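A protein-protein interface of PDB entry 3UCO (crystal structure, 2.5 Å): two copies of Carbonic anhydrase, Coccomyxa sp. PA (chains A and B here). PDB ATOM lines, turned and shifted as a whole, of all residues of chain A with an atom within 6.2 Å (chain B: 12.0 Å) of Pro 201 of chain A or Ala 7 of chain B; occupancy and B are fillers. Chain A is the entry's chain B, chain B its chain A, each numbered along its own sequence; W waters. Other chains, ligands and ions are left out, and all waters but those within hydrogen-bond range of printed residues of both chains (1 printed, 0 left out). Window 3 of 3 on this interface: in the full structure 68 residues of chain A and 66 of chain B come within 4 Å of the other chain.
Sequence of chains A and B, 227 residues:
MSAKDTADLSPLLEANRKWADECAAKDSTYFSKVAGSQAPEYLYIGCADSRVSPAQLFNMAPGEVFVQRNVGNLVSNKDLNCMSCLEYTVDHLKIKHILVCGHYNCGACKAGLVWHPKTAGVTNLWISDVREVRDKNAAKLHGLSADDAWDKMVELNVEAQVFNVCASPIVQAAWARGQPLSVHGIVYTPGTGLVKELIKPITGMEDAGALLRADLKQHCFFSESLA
Of chain B, only Ala 7 comes within 4 Å of Ser 182 of chain A.
Val 183 of chain A touches none of the printed residues of chain B.
Of the printed residues of chain B, His 184 of chain A touches Ala 7 (3.3 Å) and Leu 9 (3.5 Å).
No residue of chain B comes within 4 Å of Ile 202 of chain A.
No residue of chain B comes within 4 Å of Thr 203 of chain A.
Printed residues of chain B within 4 Å of His 97 of chain A: Ala 7.
Printed residues of chain A within 4 Å of Leu 9 of chain B: His 184 and Glu 197.
Printed residues of chain B within 4 Å of Glu 197 of chain A: Leu 9.
Thr 6 of chain B touches none of the printed residues of chain A.
The nearest residue of chain B that does not touch Pro 201 of chain A is Asp 8 of chain B (4.8 Å).
The nearest printed residue of chain B that does not touch Glu 197 of chain A is Leu 13 of chain B (4.2 Å).
Of the 13 printed residues of chain A, 5 touch a printed residue of chain B.
Printed residues of chain A that touch a printed residue of chain B: His 97, Ser 182, His 184, Glu 197 and Pro 201.
Hydrophobic or aromatic side chains of chain A within 4 Å of the printed part of chain B: His 97, His 184 and Pro 201.
Along chain A the printed residues that touch a printed residue of chain B span positions 97 to 201.
Among the printed residues, no Asp or Glu carboxylate lies within 4 Å of a Lys or Arg side-chain nitrogen of the other chain.
Water W1 bridges OE1 of Glu 197 of chain A and N of Leu 9 of chain B.
Among the printed residues, merely in contact across the chains: His 97 of chain A with Ala 7 of chain B (3.8 Å), Ser 182 of chain A with Ala 7 of chain B (3.7 Å), His 184 of chain A with Ala 7 of chain B (3.3 Å), His 184 of chain A with Leu 9 of chain B (3.5 Å), Glu 197 of chain A with Leu 9 of chain B (3.7 Å) and Pro 201 of chain A with Ala 7 of chain B (3.7 Å).
The backbone carbonyl oxygen (O) of Lys 96 of chain A is in hydrogen-bond range of the backbone NH (N) of Ser 182 of chain A, at 3.0 Å.
OG of Ser 182 of chain A sits at hydrogen-bond distance from NE2 of His 184 of chain A (2.8 Å).
No position is printed for both chains.
Of the 6 pairs that touch across the chains among the printed residues, none has its exchanged pair printed and touching as well.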
ATOM      1  N   LYS A  96      17.216  -2.403  -3.779  1.00  0.00           N
ATOM      2  CA  LYS A  96      16.942  -2.597  -5.195  1.00  0.00           C
ATOM      3  C   LYS A  96      16.973  -1.258  -5.943  1.00  0.00           C
ATOM      4  O   LYS A  96      17.125  -1.239  -7.177  1.00  0.00           O
ATOM      5  CB  LYS A  96      15.561  -3.278  -5.390  1.00  0.00           C
ATOM      6  CG  LYS A  96      15.539  -4.822  -5.404  1.00  0.00           C
ATOM      7  CD  LYS A  96      15.228  -5.475  -3.998  1.00  0.00           C
ATOM      8  CE  LYS A  96      13.931  -6.377  -3.958  1.00  0.00           C
ATOM      9  NZ  LYS A  96      12.682  -5.581  -4.209  1.00  0.00           N
ATOM     10  N   HIS A  97      16.817  -0.141  -5.208  1.00  0.00           N
ATOM     11  CA  HIS A  97      16.669   1.188  -5.861  1.00  0.00           C
ATOM     12  C   HIS A  97      17.390   2.293  -5.159  1.00  0.00           C
ATOM     13  O   HIS A  97      17.352   2.404  -3.911  1.00  0.00           O
ATOM     14  CB  HIS A  97      15.202   1.609  -5.972  1.00  0.00           C
ATOM     15  CG  HIS A  97      14.296   0.547  -6.524  1.00  0.00           C
ATOM     16  ND1 HIS A  97      13.367  -0.119  -5.749  1.00  0.00           N
ATOM     17  CD2 HIS A  97      14.172   0.047  -7.774  1.00  0.00           C
ATOM     18  CE1 HIS A  97      12.720  -0.992  -6.500  1.00  0.00           C
ATOM     19  NE2 HIS A  97      13.192  -0.909  -7.732  1.00  0.00           N
ATOM     20  N   SER A 182      18.489  -0.159  -9.639  1.00  0.00           N
ATOM     21  CA  SER A 182      18.205   0.989 -10.511  1.00  0.00           C
ATOM     22  C   SER A 182      18.543   2.283  -9.805  1.00  0.00           C
ATOM     23  O   SER A 182      18.525   2.370  -8.560  1.00  0.00           O
ATOM     24  CB  SER A 182      16.742   1.051 -10.884  1.00  0.00           C
ATOM     25  OG  SER A 182      15.959   1.112  -9.706  1.00  0.00           O
ATOM     26  N   VAL A 183      18.796   3.307 -10.604  1.00  0.00           N
ATOM     27  CA  VAL A 183      19.231   4.579 -10.099  1.00  0.00           C
ATOM     28  C   VAL A 183      18.278   5.640 -10.633  1.00  0.00           C
ATOM     29  O   VAL A 183      18.015   5.686 -11.845  1.00  0.00           O
ATOM     30  CB  VAL A 183      20.643   4.852 -10.572  1.00  0.00           C
ATOM     31  CG1 VAL A 183      21.103   6.222 -10.053  1.00  0.00           C
ATOM     32  CG2 VAL A 183      21.547   3.745 -10.092  1.00  0.00           C
ATOM     33  N   HIS A 184      17.796   6.506  -9.742  1.00  0.00           N
ATOM     34  CA  HIS A 184      16.772   7.494 -10.094  1.00  0.00           C
ATOM     35  C   HIS A 184      17.186   8.909  -9.776  1.00  0.00           C
ATOM     36  O   HIS A 184      17.593   9.175  -8.645  1.00  0.00           O
ATOM     37  CB  HIS A 184      15.536   7.198  -9.261  1.00  0.00           C
ATOM     38  CG  HIS A 184      15.042   5.814  -9.452  1.00  0.00           C
ATOM     39  ND1 HIS A 184      14.187   5.478 -10.479  1.00  0.00           N
ATOM     40  CD2 HIS A 184      15.383   4.653  -8.832  1.00  0.00           C
ATOM     41  CE1 HIS A 184      13.987   4.172 -10.447  1.00  0.00           C
ATOM     42  NE2 HIS A 184      14.711   3.648  -9.468  1.00  0.00           N
ATOM     43  N   GLU A 197      10.340  13.597 -11.201  1.00  0.00           N
ATOM     44  CA  GLU A 197      11.328  12.738 -11.790  1.00  0.00           C
ATOM     45  C   GLU A 197      12.149  13.428 -12.883  1.00  0.00           C
ATOM     46  O   GLU A 197      11.597  13.758 -13.895  1.00  0.00           O
ATOM     47  CB  GLU A 197      10.586  11.593 -12.396  1.00  0.00           C
ATOM     48  CG  GLU A 197      11.433  10.595 -13.092  1.00  0.00           C
ATOM     49  CD  GLU A 197      10.668   9.305 -13.209  1.00  0.00           C
ATOM     50  OE1 GLU A 197      11.221   8.233 -12.942  1.00  0.00           O
ATOM     51  OE2 GLU A 197       9.468   9.382 -13.527  1.00  0.00           O
ATOM     52  N   ILE A 199      15.260  12.224 -14.234  1.00  0.00           N
ATOM     53  CA  ILE A 199      15.932  11.248 -15.061  1.00  0.00           C
ATOM     54  C   ILE A 199      15.152   9.974 -14.851  1.00  0.00           C
ATOM     55  O   ILE A 199      14.887   9.539 -13.705  1.00  0.00           O
ATOM     56  CB  ILE A 199      17.414  11.057 -14.654  1.00  0.00           C
ATOM     57  CG1 ILE A 199      18.150  12.402 -14.689  1.00  0.00           C
ATOM     58  CG2 ILE A 199      18.095   9.992 -15.543  1.00  0.00           C
ATOM     59  CD1 ILE A 199      19.666  12.311 -14.662  1.00  0.00           C
ATOM     60  N   LYS A 200      14.716   9.422 -15.977  1.00  0.00           N
ATOM     61  CA  LYS A 200      13.966   8.164 -15.972  1.00  0.00           C
ATOM     62  C   LYS A 200      14.898   7.028 -15.443  1.00  0.00           C
ATOM     63  O   LYS A 200      16.136   7.142 -15.553  1.00  0.00           O
ATOM     64  CB  LYS A 200      13.418   7.892 -17.396  1.00  0.00           C
ATOM     65  CG  LYS A 200      12.141   8.683 -17.781  1.00  0.00           C
ATOM     66  CD  LYS A 200      10.913   8.030 -16.999  1.00  0.00           C
ATOM     67  CE  LYS A 200       9.482   8.384 -17.528  1.00  0.00           C
ATOM     68  NZ  LYS A 200       9.496   8.847 -18.990  1.00  0.00           N
ATOM     69  N   PRO A 201      14.311   5.940 -14.878  1.00  0.00           N
ATOM     70  CA  PRO A 201      15.084   4.858 -14.240  1.00  0.00           C
ATOM     71  C   PRO A 201      16.272   4.389 -15.075  1.00  0.00           C
ATOM     72  O   PRO A 201      16.153   4.199 -16.287  1.00  0.00           O
ATOM     73  CB  PRO A 201      14.061   3.721 -14.105  1.00  0.00           C
ATOM     74  CG  PRO A 201      12.754   4.488 -13.923  1.00  0.00           C
ATOM     75  CD  PRO A 201      12.885   5.592 -14.944  1.00  0.00           C
ATOM     76  N   ILE A 202      17.421   4.240 -14.427  1.00  0.00           N
ATOM     77  CA  ILE A 202      18.565   3.642 -15.053  1.00  0.00           C
ATOM     78  C   ILE A 202      18.734   2.248 -14.419  1.00  0.00           C
ATOM     79  O   ILE A 202      18.831   2.125 -13.195  1.00  0.00           O
ATOM     80  CB  ILE A 202      19.775   4.552 -14.930  1.00  0.00           C
ATOM     81  CG1 ILE A 202      19.577   5.795 -15.832  1.00  0.00           C
ATOM     82  CG2 ILE A 202      21.021   3.836 -15.377  1.00  0.00           C
ATOM     83  CD1 ILE A 202      20.519   7.000 -15.540  1.00  0.00           C
ATOM     84  N   THR A 203      18.738   1.203 -15.248  1.00  0.00           N
ATOM     85  CA  THR A 203      18.849  -0.184 -14.710  1.00  0.00           C
ATOM     86  C   THR A 203      20.135  -0.891 -15.121  1.00  0.00           C
ATOM     87  O   THR A 203      20.398  -1.987 -14.630  1.00  0.00           O
ATOM     88  CB  THR A 203      17.625  -1.125 -15.070  1.00  0.00           C
ATOM     89  OG1 THR A 203      17.519  -1.238 -16.493  1.00  0.00           O
ATOM     90  CG2 THR A 203      16.349  -0.564 -14.568  1.00  0.00           C
ATOM     91  N   ASP A 207      20.457   1.585 -20.515  1.00  0.00           N
ATOM     92  CA  ASP A 207      19.705   2.740 -20.039  1.00  0.00           C
ATOM     93  C   ASP A 207      20.595   4.025 -19.880  1.00  0.00           C
ATOM     94  O   ASP A 207      20.224   5.109 -20.319  1.00  0.00           O
ATOM     95  CB  ASP A 207      19.033   2.392 -18.693  1.00  0.00           C
ATOM     96  CG  ASP A 207      17.818   1.466 -18.838  1.00  0.00           C
ATOM     97  OD1 ASP A 207      17.441   1.117 -19.971  1.00  0.00           O
ATOM     98  OD2 ASP A 207      17.207   1.100 -17.817  1.00  0.00           O
ATOM     99  N   LEU A 211      20.112   7.890 -21.348  1.00  0.00           N
ATOM    100  CA  LEU A 211      19.516   8.899 -20.486  1.00  0.00           C
ATOM    101  C   LEU A 211      20.469   9.942 -19.951  1.00  0.00           C
ATOM    102  O   LEU A 211      20.035  10.997 -19.465  1.00  0.00           O
ATOM    103  CB  LEU A 211      18.773   8.209 -19.344  1.00  0.00           C
ATOM    104  CG  LEU A 211      17.569   7.408 -19.853  1.00  0.00           C
ATOM    105  CD1 LEU A 211      17.032   6.431 -18.832  1.00  0.00           C
ATOM    106  CD2 LEU A 211      16.490   8.434 -20.293  1.00  0.00           C
ATOM    107  N   THR B   6       9.304  -1.487 -15.110  1.00  0.00           N
ATOM    108  CA  THR B   6      10.028  -2.596 -14.395  1.00  0.00           C
ATOM    109  C   THR B   6      10.341  -2.130 -12.924  1.00  0.00           C
ATOM    110  O   THR B   6       9.823  -2.709 -11.921  1.00  0.00           O
ATOM    111  CB  THR B   6      11.294  -3.155 -15.253  1.00  0.00           C
ATOM    112  OG1 THR B   6      12.158  -3.980 -14.451  1.00  0.00           O
ATOM    113  CG2 THR B   6      12.146  -2.001 -15.953  1.00  0.00           C
ATOM    114  N   ALA B   7      11.148  -1.054 -12.852  1.00  0.00           N
ATOM    115  CA  ALA B   7      11.442  -0.293 -11.644  1.00  0.00           C
ATOM    116  C   ALA B   7      10.844   1.158 -11.689  1.00  0.00           C
ATOM    117  O   ALA B   7      11.524   2.129 -11.410  1.00  0.00           O
ATOM    118  CB  ALA B   7      12.940  -0.236 -11.463  1.00  0.00           C
ATOM    119  N   ASP B   8       9.579   1.269 -12.069  1.00  0.00           N
ATOM    120  CA  ASP B   8       8.771   2.488 -12.039  1.00  0.00           C
ATOM    121  C   ASP B   8       8.701   3.209 -10.647  1.00  0.00           C
ATOM    122  O   ASP B   8       8.563   2.556  -9.598  1.00  0.00           O
ATOM    123  CB  ASP B   8       7.349   2.044 -12.486  1.00  0.00           C
ATOM    124  CG  ASP B   8       6.397   3.207 -12.806  1.00  0.00           C
ATOM    125  OD1 ASP B   8       6.367   4.236 -12.104  1.00  0.00           O
ATOM    126  OD2 ASP B   8       5.620   3.051 -13.770  1.00  0.00           O
ATOM    127  N   LEU B   9       8.756   4.546 -10.644  1.00  0.00           N
ATOM    128  CA  LEU B   9       8.573   5.312  -9.389  1.00  0.00           C
ATOM    129  C   LEU B   9       7.157   5.816  -9.084  1.00  0.00           C
ATOM    130  O   LEU B   9       6.932   6.416  -8.025  1.00  0.00           O
ATOM    131  CB  LEU B   9       9.501   6.525  -9.318  1.00  0.00           C
ATOM    132  CG  LEU B   9      11.006   6.388  -9.223  1.00  0.00           C
ATOM    133  CD1 LEU B   9      11.550   7.773  -9.330  1.00  0.00           C
ATOM    134  CD2 LEU B   9      11.426   5.710  -7.957  1.00  0.00           C
ATOM    135  N   SER B  10       6.226   5.586 -10.008  1.00  0.00           N
ATOM    136  CA  SER B  10       4.821   6.023  -9.882  1.00  0.00           C
ATOM    137  C   SER B  10       4.174   5.937  -8.497  1.00  0.00           C
ATOM    138  O   SER B  10       3.566   6.909  -8.058  1.00  0.00           O
ATOM    139  CB  SER B  10       3.952   5.295 -10.897  1.00  0.00           C
ATOM    140  OG  SER B  10       4.051   5.987 -12.122  1.00  0.00           O
ATOM    141  N   PRO B  11       4.298   4.786  -7.817  1.00  0.00           N
ATOM    142  CA  PRO B  11       3.720   4.681  -6.474  1.00  0.00           C
ATOM    143  C   PRO B  11       4.347   5.601  -5.439  1.00  0.00           C
ATOM    144  O   PRO B  11       3.678   5.995  -4.461  1.00  0.00           O
ATOM    145  CB  PRO B  11       3.950   3.220  -6.083  1.00  0.00           C
ATOM    146  CG  PRO B  11       4.855   2.638  -7.190  1.00  0.00           C
ATOM    147  CD  PRO B  11       4.608   3.475  -8.393  1.00  0.00           C
ATOM    148  N   LEU B  12       5.623   5.922  -5.616  1.00  0.00           N
ATOM    149  CA  LEU B  12       6.266   6.884  -4.729  1.00  0.00           C
ATOM    150  C   LEU B  12       5.767   8.276  -5.040  1.00  0.00           C
ATOM    151  O   LEU B  12       5.443   9.030  -4.099  1.00  0.00           O
ATOM    152  CB  LEU B  12       7.782   6.848  -4.870  1.00  0.00           C
ATOM    153  CG  LEU B  12       8.513   5.726  -4.163  1.00  0.00           C
ATOM    154  CD1 LEU B  12       9.924   6.106  -4.144  1.00  0.00           C
ATOM    155  CD2 LEU B  12       8.022   5.569  -2.741  1.00  0.00           C
ATOM    156  N   LEU B  13       5.689   8.605  -6.336  1.00  0.00           N
ATOM    157  CA  LEU B  13       5.144   9.885  -6.767  1.00  0.00           C
ATOM    158  C   LEU B  13       3.652  10.095  -6.359  1.00  0.00           C
ATOM    159  O   LEU B  13       3.325  11.186  -5.826  1.00  0.00           O
ATOM    160  CB  LEU B  13       5.392  10.147  -8.247  1.00  0.00           C
ATOM    161  CG  LEU B  13       6.848   9.985  -8.757  1.00  0.00           C
ATOM    162  CD1 LEU B  13       6.919  10.024 -10.261  1.00  0.00           C
ATOM    163  CD2 LEU B  13       7.845  10.966  -8.149  1.00  0.00           C
HETATM  164  O   HOH W   1       9.708   5.962 -13.089  1.00  0.00           O
